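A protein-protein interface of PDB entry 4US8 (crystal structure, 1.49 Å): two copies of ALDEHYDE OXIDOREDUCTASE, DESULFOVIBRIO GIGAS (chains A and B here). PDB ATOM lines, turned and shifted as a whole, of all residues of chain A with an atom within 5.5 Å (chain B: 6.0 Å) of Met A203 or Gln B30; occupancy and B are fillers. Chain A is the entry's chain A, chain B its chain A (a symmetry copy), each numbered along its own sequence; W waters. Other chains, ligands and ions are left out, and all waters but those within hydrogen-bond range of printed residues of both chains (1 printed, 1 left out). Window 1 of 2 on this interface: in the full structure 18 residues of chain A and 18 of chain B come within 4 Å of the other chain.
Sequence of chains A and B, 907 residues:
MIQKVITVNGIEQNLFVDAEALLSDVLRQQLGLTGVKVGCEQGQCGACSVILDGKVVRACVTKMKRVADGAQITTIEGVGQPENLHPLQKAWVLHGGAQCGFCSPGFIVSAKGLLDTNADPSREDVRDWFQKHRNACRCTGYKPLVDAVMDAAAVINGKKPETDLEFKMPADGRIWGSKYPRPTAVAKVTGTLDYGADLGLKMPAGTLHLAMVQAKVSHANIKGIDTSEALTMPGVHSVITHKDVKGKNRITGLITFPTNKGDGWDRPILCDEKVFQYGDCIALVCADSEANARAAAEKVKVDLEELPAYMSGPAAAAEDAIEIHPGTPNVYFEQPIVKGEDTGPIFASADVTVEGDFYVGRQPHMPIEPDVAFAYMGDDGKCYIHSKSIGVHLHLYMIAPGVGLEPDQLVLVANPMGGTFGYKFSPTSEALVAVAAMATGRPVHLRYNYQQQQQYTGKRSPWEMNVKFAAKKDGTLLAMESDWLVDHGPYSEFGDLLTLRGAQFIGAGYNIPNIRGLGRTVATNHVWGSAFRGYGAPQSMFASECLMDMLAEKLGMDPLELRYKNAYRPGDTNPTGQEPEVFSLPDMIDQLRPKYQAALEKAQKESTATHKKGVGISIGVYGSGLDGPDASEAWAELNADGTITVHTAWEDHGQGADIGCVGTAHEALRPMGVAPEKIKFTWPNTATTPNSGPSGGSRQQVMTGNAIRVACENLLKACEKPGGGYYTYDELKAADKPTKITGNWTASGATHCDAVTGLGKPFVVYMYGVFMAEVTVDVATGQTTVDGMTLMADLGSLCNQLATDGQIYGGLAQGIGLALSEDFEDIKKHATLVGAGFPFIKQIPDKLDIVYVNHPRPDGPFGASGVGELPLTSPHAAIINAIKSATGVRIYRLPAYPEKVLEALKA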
ATOM      1  N   LEU A 199     -26.505  22.902   5.803  1.00  0.00           N
ATOM      2  CA  LEU A 199     -27.543  21.860   5.811  1.00  0.00           C
ATOM      3  C   LEU A 199     -27.097  20.651   4.994  1.00  0.00           C
ATOM      4  O   LEU A 199     -27.315  19.500   5.400  1.00  0.00           O
ATOM      5  CB  LEU A 199     -28.898  22.420   5.338  1.00  0.00           C
ATOM      6  CG  LEU A 199     -29.485  23.479   6.273  1.00  0.00           C
ATOM      7  CD1 LEU A 199     -30.660  24.195   5.624  1.00  0.00           C
ATOM      8  CD2 LEU A 199     -29.895  22.910   7.633  1.00  0.00           C
ATOM      9  N   GLY A 200     -26.498  20.893   3.832  1.00  0.00           N
ATOM     10  CA  GLY A 200     -25.985  19.805   3.005  1.00  0.00           C
ATOM     11  C   GLY A 200     -25.008  18.878   3.740  1.00  0.00           C
ATOM     12  O   GLY A 200     -25.041  17.672   3.574  1.00  0.00           O
ATOM     13  N   LEU A 201     -24.152  19.442   4.576  1.00  0.00           N
ATOM     14  CA  LEU A 201     -23.208  18.638   5.342  1.00  0.00           C
ATOM     15  C   LEU A 201     -23.893  17.828   6.445  1.00  0.00           C
ATOM     16  O   LEU A 201     -23.334  16.849   6.949  1.00  0.00           O
ATOM     17  CB  LEU A 201     -22.137  19.546   5.948  1.00  0.00           C
ATOM     18  CG  LEU A 201     -21.148  20.165   4.969  1.00  0.00           C
ATOM     19  CD1 LEU A 201     -20.064  20.944   5.709  1.00  0.00           C
ATOM     20  CD2 LEU A 201     -20.525  19.146   4.027  1.00  0.00           C
ATOM     21  N   LYS A 202     -25.094  18.244   6.826  1.00  0.00           N
ATOM     22  CA  LYS A 202     -25.820  17.622   7.933  1.00  0.00           C
ATOM     23  C   LYS A 202     -27.000  16.776   7.470  1.00  0.00           C
ATOM     24  O   LYS A 202     -27.860  16.400   8.294  1.00  0.00           O
ATOM     25  CB  LYS A 202     -26.285  18.709   8.907  1.00  0.00           C
ATOM     26  CG  LYS A 202     -25.131  19.547   9.445  1.00  0.00           C
ATOM     27  CD  LYS A 202     -25.537  20.669  10.383  1.00  0.00           C
ATOM     28  CE  LYS A 202     -24.325  21.452  10.805  1.00  0.00           C
ATOM     29  NZ  LYS A 202     -24.655  22.456  11.840  1.00  0.00           N
ATOM     30  N   MET A 203     -27.052  16.505   6.171  1.00  0.00           N
ATOM     31  CA  MET A 203     -28.084  15.658   5.597  1.00  0.00           C
ATOM     32  C   MET A 203     -27.617  14.212   5.726  1.00  0.00           C
ATOM     33  O   MET A 203     -26.421  13.911   5.925  1.00  0.00           O
ATOM     34  CB  MET A 203     -28.367  16.040   4.130  1.00  0.00           C
ATOM     35  CG  MET A 203     -29.253  17.278   4.013  1.00  0.00           C
ATOM     36  SD  MET A 203     -29.458  17.933   2.350  1.00  0.00           S
ATOM     37  CE  MET A 203     -30.737  16.856   1.768  1.00  0.00           C
ATOM     38  N   PRO A 204     -28.536  13.302   5.559  1.00  0.00           N
ATOM     39  CA  PRO A 204     -28.133  11.904   5.792  1.00  0.00           C
ATOM     40  C   PRO A 204     -27.308  11.273   4.697  1.00  0.00           C
ATOM     41  O   PRO A 204     -27.312  11.749   3.596  1.00  0.00           O
ATOM     42  CB  PRO A 204     -29.443  11.172   5.917  1.00  0.00           C
ATOM     43  CG  PRO A 204     -30.471  12.002   5.334  1.00  0.00           C
ATOM     44  CD  PRO A 204     -29.962  13.451   5.288  1.00  0.00           C
ATOM     45  N   ALA A 205     -26.730  10.112   5.011  1.00  0.00           N
ATOM     46  CA  ALA A 205     -25.846   9.378   4.103  1.00  0.00           C
ATOM     47  C   ALA A 205     -26.440   9.107   2.722  1.00  0.00           C
ATOM     48  O   ALA A 205     -25.712   9.120   1.739  1.00  0.00           O
ATOM     49  CB  ALA A 205     -25.405   8.067   4.751  1.00  0.00           C
ATOM     50  N   THR A 207     -28.086  10.960   0.820  1.00  0.00           N
ATOM     51  CA  THR A 207     -28.239  12.184   0.024  1.00  0.00           C
ATOM     52  C   THR A 207     -27.264  12.154  -1.153  1.00  0.00           C
ATOM     53  O   THR A 207     -26.089  11.808  -1.002  1.00  0.00           O
ATOM     54  CB  THR A 207     -27.983  13.410   0.896  1.00  0.00           C
ATOM     55  OG1 THR A 207     -28.922  13.425   1.985  1.00  0.00           O
ATOM     56  CG2 THR A 207     -28.117  14.717   0.091  1.00  0.00           C
ATOM     57  N   PHE A 374     -31.549  22.338  -2.080  1.00  0.00           N
ATOM     58  CA  PHE A 374     -31.723  20.905  -1.985  1.00  0.00           C
ATOM     59  C   PHE A 374     -33.170  20.532  -2.111  1.00  0.00           C
ATOM     60  O   PHE A 374     -34.036  21.383  -1.965  1.00  0.00           O
ATOM     61  CB  PHE A 374     -31.025  20.321  -0.735  1.00  0.00           C
ATOM     62  CG  PHE A 374     -31.517  20.833   0.586  1.00  0.00           C
ATOM     63  CD1 PHE A 374     -32.550  20.181   1.250  1.00  0.00           C
ATOM     64  CD2 PHE A 374     -30.920  21.901   1.198  1.00  0.00           C
ATOM     65  CE1 PHE A 374     -32.986  20.614   2.486  1.00  0.00           C
ATOM     66  CE2 PHE A 374     -31.346  22.337   2.434  1.00  0.00           C
ATOM     67  CZ  PHE A 374     -32.360  21.687   3.096  1.00  0.00           C
ATOM     68  N   ALA A 375     -33.430  19.247  -2.368  1.00  0.00           N
ATOM     69  CA  ALA A 375     -34.802  18.782  -2.536  1.00  0.00           C
ATOM     70  C   ALA A 375     -34.882  17.340  -2.128  1.00  0.00           C
ATOM     71  O   ALA A 375     -33.873  16.615  -2.120  1.00  0.00           O
ATOM     72  CB  ALA A 375     -35.280  18.930  -3.966  1.00  0.00           C
ATOM     73  N   TYR A 376     -36.097  16.909  -1.824  1.00  0.00           N
ATOM     74  CA  TYR A 376     -36.334  15.515  -1.440  1.00  0.00           C
ATOM     75  C   TYR A 376     -37.809  15.196  -1.624  1.00  0.00           C
ATOM     76  O   TYR A 376     -38.640  16.083  -1.684  1.00  0.00           O
ATOM     77  CB  TYR A 376     -35.888  15.256   0.024  1.00  0.00           C
ATOM     78  CG  TYR A 376     -36.511  16.194   1.030  1.00  0.00           C
ATOM     79  CD1 TYR A 376     -37.729  15.891   1.627  1.00  0.00           C
ATOM     80  CD2 TYR A 376     -35.917  17.416   1.359  1.00  0.00           C
ATOM     81  CE1 TYR A 376     -38.346  16.772   2.514  1.00  0.00           C
ATOM     82  CE2 TYR A 376     -36.522  18.294   2.252  1.00  0.00           C
ATOM     83  CZ  TYR A 376     -37.736  17.985   2.814  1.00  0.00           C
ATOM     84  OH  TYR A 376     -38.309  18.874   3.687  1.00  0.00           O
ATOM     85  N   PRO A 443     -32.940  12.215  -1.596  1.00  0.00           N
ATOM     86  CA  PRO A 443     -32.586  13.601  -1.351  1.00  0.00           C
ATOM     87  C   PRO A 443     -31.395  13.999  -2.227  1.00  0.00           C
ATOM     88  O   PRO A 443     -30.467  13.180  -2.465  1.00  0.00           O
ATOM     89  CB  PRO A 443     -32.212  13.628   0.143  1.00  0.00           C
ATOM     90  CG  PRO A 443     -32.797  12.373   0.713  1.00  0.00           C
ATOM     91  CD  PRO A 443     -32.707  11.390  -0.398  1.00  0.00           C
ATOM     92  N   VAL A 444     -31.432  15.247  -2.705  1.00  0.00           N
ATOM     93  CA  VAL A 444     -30.384  15.784  -3.547  1.00  0.00           C
ATOM     94  C   VAL A 444     -29.988  17.162  -3.071  1.00  0.00           C
ATOM     95  O   VAL A 444     -30.822  17.919  -2.584  1.00  0.00           O
ATOM     96  CB  VAL A 444     -30.799  15.831  -5.038  1.00  0.00           C
ATOM     97  CG1 VAL A 444     -31.193  14.424  -5.518  1.00  0.00           C
ATOM     98  CG2 VAL A 444     -31.940  16.831  -5.279  1.00  0.00           C
ATOM     99  N   HIS A 445     -28.713  17.485  -3.245  1.00  0.00           N
ATOM    100  CA  HIS A 445     -28.173  18.776  -2.810  1.00  0.00           C
ATOM    101  C   HIS A 445     -27.243  19.327  -3.888  1.00  0.00           C
ATOM    102  O   HIS A 445     -26.393  18.584  -4.401  1.00  0.00           O
ATOM    103  CB  HIS A 445     -27.430  18.610  -1.466  1.00  0.00           C
ATOM    104  CG  HIS A 445     -26.976  19.892  -0.858  1.00  0.00           C
ATOM    105  ND1 HIS A 445     -25.815  20.525  -1.230  1.00  0.00           N
ATOM    106  CD2 HIS A 445     -27.508  20.632   0.127  1.00  0.00           C
ATOM    107  CE1 HIS A 445     -25.660  21.623  -0.519  1.00  0.00           C
ATOM    108  NE2 HIS A 445     -26.688  21.722   0.307  1.00  0.00           N
ATOM    109  N   MET B   1     -37.995  11.449   3.233  1.00  0.00           N
ATOM    110  CA  MET B   1     -37.194  12.322   4.145  1.00  0.00           C
ATOM    111  C   MET B   1     -38.157  13.311   4.779  1.00  0.00           C
ATOM    112  O   MET B   1     -39.205  13.645   4.187  1.00  0.00           O
ATOM    113  CB  MET B   1     -36.108  13.075   3.345  1.00  0.00           C
ATOM    114  CG  MET B   1     -35.511  14.301   4.054  1.00  0.00           C
ATOM    115  SD  MET B   1     -34.039  14.924   3.243  1.00  0.00           S
ATOM    116  CE  MET B   1     -32.796  13.840   3.873  1.00  0.00           C
ATOM    117  N   LEU B  15     -33.353  20.065  11.158  1.00  0.00           N
ATOM    118  CA  LEU B  15     -32.854  18.721  10.818  1.00  0.00           C
ATOM    119  C   LEU B  15     -33.558  18.140   9.652  1.00  0.00           C
ATOM    120  O   LEU B  15     -34.784  18.250   9.520  1.00  0.00           O
ATOM    121  CB  LEU B  15     -33.019  17.720  11.955  1.00  0.00           C
ATOM    122  CG  LEU B  15     -32.219  17.846  13.195  1.00  0.00           C
ATOM    123  CD1 LEU B  15     -32.623  16.668  14.108  1.00  0.00           C
ATOM    124  CD2 LEU B  15     -30.756  17.811  12.793  1.00  0.00           C
ATOM    125  N   PHE B  16     -32.777  17.454   8.835  1.00  0.00           N
ATOM    126  CA  PHE B  16     -33.306  16.698   7.707  1.00  0.00           C
ATOM    127  C   PHE B  16     -32.900  15.248   7.846  1.00  0.00           C
ATOM    128  O   PHE B  16     -31.716  14.919   7.841  1.00  0.00           O
ATOM    129  CB  PHE B  16     -32.764  17.323   6.426  1.00  0.00           C
ATOM    130  CG  PHE B  16     -33.325  18.707   6.216  1.00  0.00           C
ATOM    131  CD1 PHE B  16     -34.538  18.882   5.577  1.00  0.00           C
ATOM    132  CD2 PHE B  16     -32.697  19.796   6.784  1.00  0.00           C
ATOM    133  CE1 PHE B  16     -35.079  20.143   5.456  1.00  0.00           C
ATOM    134  CE2 PHE B  16     -33.261  21.052   6.695  1.00  0.00           C
ATOM    135  CZ  PHE B  16     -34.451  21.221   6.035  1.00  0.00           C
ATOM    136  N   VAL B  17     -33.901  14.404   8.022  1.00  0.00           N
ATOM    137  CA  VAL B  17     -33.676  13.031   8.414  1.00  0.00           C
ATOM    138  C   VAL B  17     -34.612  12.066   7.719  1.00  0.00           C
ATOM    139  O   VAL B  17     -35.692  12.438   7.257  1.00  0.00           O
ATOM    140  CB  VAL B  17     -33.856  12.835   9.948  1.00  0.00           C
ATOM    141  CG1 VAL B  17     -32.769  13.580  10.725  1.00  0.00           C
ATOM    142  CG2 VAL B  17     -35.256  13.223  10.432  1.00  0.00           C
ATOM    143  N   ASP B  18     -34.166  10.814   7.666  1.00  0.00           N
ATOM    144  CA  ASP B  18     -35.050   9.703   7.358  1.00  0.00           C
ATOM    145  C   ASP B  18     -35.801   9.339   8.659  1.00  0.00           C
ATOM    146  O   ASP B  18     -35.206   9.186   9.728  1.00  0.00           O
ATOM    147  CB  ASP B  18     -34.295   8.509   6.811  1.00  0.00           C
ATOM    148  CG  ASP B  18     -35.219   7.542   6.115  1.00  0.00           C
ATOM    149  OD1 ASP B  18     -35.464   7.715   4.898  1.00  0.00           O
ATOM    150  OD2 ASP B  18     -35.734   6.634   6.800  1.00  0.00           O
ATOM    151  N   ALA B  21     -34.386   6.472  10.454  1.00  0.00           N
ATOM    152  CA  ALA B  21     -33.003   6.519  10.924  1.00  0.00           C
ATOM    153  C   ALA B  21     -32.959   6.465  12.432  1.00  0.00           C
ATOM    154  O   ALA B  21     -33.876   6.940  13.105  1.00  0.00           O
ATOM    155  CB  ALA B  21     -32.305   7.772  10.436  1.00  0.00           C
ATOM    156  N   ASP B  25     -27.330   7.521  15.140  1.00  0.00           N
ATOM    157  CA  ASP B  25     -26.653   7.851  13.892  1.00  0.00           C
ATOM    158  C   ASP B  25     -26.858   9.303  13.518  1.00  0.00           C
ATOM    159  O   ASP B  25     -25.926   9.974  13.076  1.00  0.00           O
ATOM    160  CB  ASP B  25     -27.149   6.973  12.749  1.00  0.00           C
ATOM    161  CG  ASP B  25     -26.722   5.527  12.884  1.00  0.00           C
ATOM    162  OD1 ASP B  25     -25.635   5.248  13.437  1.00  0.00           O
ATOM    163  OD2 ASP B  25     -27.484   4.660  12.435  1.00  0.00           O
ATOM    164  N   VAL B  26     -28.078   9.808  13.694  1.00  0.00           N
ATOM    165  CA  VAL B  26     -28.339  11.220  13.380  1.00  0.00           C
ATOM    166  C   VAL B  26     -27.433  12.113  14.241  1.00  0.00           C
ATOM    167  O   VAL B  26     -26.772  13.018  13.746  1.00  0.00           O
ATOM    168  CB  VAL B  26     -29.820  11.569  13.551  1.00  0.00           C
ATOM    169  CG1 VAL B  26     -30.042  13.066  13.421  1.00  0.00           C
ATOM    170  CG2 VAL B  26     -30.654  10.758  12.556  1.00  0.00           C
ATOM    171  N   LEU B  27     -27.433  11.871  15.545  1.00  0.00           N
ATOM    172  CA  LEU B  27     -26.645  12.707  16.469  1.00  0.00           C
ATOM    173  C   LEU B  27     -25.137  12.598  16.177  1.00  0.00           C
ATOM    174  O   LEU B  27     -24.462  13.602  16.076  1.00  0.00           O
ATOM    175  CB  LEU B  27     -26.949  12.360  17.925  1.00  0.00           C
ATOM    176  CG  LEU B  27     -28.389  12.631  18.389  1.00  0.00           C
ATOM    177  CD1 LEU B  27     -28.620  12.097  19.789  1.00  0.00           C
ATOM    178  CD2 LEU B  27     -28.747  14.105  18.316  1.00  0.00           C
ATOM    179  N   ARG B  28     -24.631  11.378  16.040  1.00  0.00           N
ATOM    180  CA  ARG B  28     -23.192  11.190  15.834  1.00  0.00           C
ATOM    181  C   ARG B  28     -22.725  11.633  14.455  1.00  0.00           C
ATOM    182  O   ARG B  28     -21.718  12.334  14.345  1.00  0.00           O
ATOM    183  CB  ARG B  28     -22.795   9.729  16.017  1.00  0.00           C
ATOM    184  CG  ARG B  28     -22.886   9.229  17.459  1.00  0.00           C
ATOM    185  CD  ARG B  28     -22.622   7.731  17.612  1.00  0.00           C
ATOM    186  NE  ARG B  28     -21.328   7.316  17.072  1.00  0.00           N
ATOM    187  CZ  ARG B  28     -20.155   7.551  17.659  1.00  0.00           C
ATOM    188  NH1 ARG B  28     -20.077   8.155  18.839  1.00  0.00           N
ATOM    189  NH2 ARG B  28     -19.037   7.149  17.070  1.00  0.00           N
ATOM    190  N   GLN B  29     -23.432  11.180  13.413  1.00  0.00           N
ATOM    191  CA  GLN B  29     -22.963  11.352  12.031  1.00  0.00           C
ATOM    192  C   GLN B  29     -23.426  12.676  11.430  1.00  0.00           C
ATOM    193  O   GLN B  29     -22.622  13.426  10.868  1.00  0.00           O
ATOM    194  CB  GLN B  29     -23.405  10.184  11.174  1.00  0.00           C
ATOM    195  CG  GLN B  29     -22.922   8.864  11.708  1.00  0.00           C
ATOM    196  CD  GLN B  29     -23.186   7.715  10.792  1.00  0.00           C
ATOM    197  OE1 GLN B  29     -23.048   7.827   9.583  1.00  0.00           O
ATOM    198  NE2 GLN B  29     -23.507   6.579  11.374  1.00  0.00           N
ATOM    199  N   GLN B  30     -24.715  12.980  11.536  1.00  0.00           N
ATOM    200  CA  GLN B  30     -25.226  14.214  10.937  1.00  0.00           C
ATOM    201  C   GLN B  30     -24.831  15.440  11.750  1.00  0.00           C
ATOM    202  O   GLN B  30     -24.462  16.473  11.161  1.00  0.00           O
ATOM    203  CB  GLN B  30     -26.748  14.151  10.704  1.00  0.00           C
ATOM    204  CG  GLN B  30     -27.119  13.092   9.674  1.00  0.00           C
ATOM    205  CD  GLN B  30     -28.592  12.973   9.422  1.00  0.00           C
ATOM    206  OE1 GLN B  30     -29.185  11.889   9.608  1.00  0.00           O
ATOM    207  NE2 GLN B  30     -29.210  14.062   8.987  1.00  0.00           N
ATOM    208  N   LEU B  31     -24.890  15.328  13.086  1.00  0.00           N
ATOM    209  CA  LEU B  31     -24.597  16.479  13.952  1.00  0.00           C
ATOM    210  C   LEU B  31     -23.224  16.489  14.618  1.00  0.00           C
ATOM    211  O   LEU B  31     -22.895  17.442  15.295  1.00  0.00           O
ATOM    212  CB  LEU B  31     -25.676  16.645  15.017  1.00  0.00           C
ATOM    213  CG  LEU B  31     -27.114  16.796  14.477  1.00  0.00           C
ATOM    214  CD1 LEU B  31     -28.119  17.046  15.594  1.00  0.00           C
ATOM    215  CD2 LEU B  31     -27.229  17.889  13.404  1.00  0.00           C
ATOM    216  N   GLY B  32     -22.446  15.431  14.448  1.00  0.00           N
ATOM    217  CA  GLY B  32     -21.086  15.377  14.974  1.00  0.00           C
ATOM    218  C   GLY B  32     -21.008  15.205  16.485  1.00  0.00           C
ATOM    219  O   GLY B  32     -19.953  15.452  17.061  1.00  0.00           O
HETATM  220  O   HOH W   1     -29.949  18.078   9.163  1.00  0.00           O
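NE2 of Gln B30 lies within hydrogen-bond range of O of Lys A202 (2.8 Å).
OG1 of Thr A207 sits at hydrogen-bond distance from O of Pro A204 (2.8 Å).
The side-chain amide nitrogen (NE2) of Gln B30 is in hydrogen-bond range of the backbone carbonyl oxygen (O) of Phe B16, 2.9 Å away.
Among the printed residues, pairs that only touch across the chains: Pro A204 with Met B1, Pro A204 with Phe B16, Pro A443 with Met B1, Tyr A376 with Met B1, Pro A204 with Gln B30, Met A203 with Gln B30, Phe A374 with Phe B16, Tyr A376 with Phe B16 and Leu A199 with Phe B16.
Met A203 touches just one residue of chain B: Gln B30.
Of the printed residues of chain B, Phe A374 touches Phe B16 (3.6 Å).
Of the printed residues of chain A, Phe B16 touches Leu A199, Pro A204, Phe A374 and Tyr A376.
Val B17 touches none of the printed residues of chain A.
Gln B29 touches none of the printed residues of chain A.
The nearest residue of chain A that does not touch Gln B30 is Leu A201 (4.4 Å).
The nearest printed residue of chain B that does not touch Pro A204 is Asp B18 (4.5 Å).
Of the 14 printed residues of chain A, 7 touch a printed residue of chain B.
Hydrophobic or aromatic side chains of chain A that line the printed part of chain B: Leu A199, Pro A204, Phe A374, Tyr A376 and Pro A443.
Printed residues of chain B that touch a printed residue of chain A: Met B1, Phe B16 and Gln B30.
Hydrophobic or aromatic side chains of chain B that line the printed part of chain A: Met B1 and Phe B16.
Among the printed residues, no Asp or Glu carboxylate lies within 4 Å of a Lys or Arg side-chain nitrogen of the other chain.
No position is printed for both chains.
Water W1 bridges O of Lys A202 (2.8 Å) and N of Phe B16 (2.9 Å).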
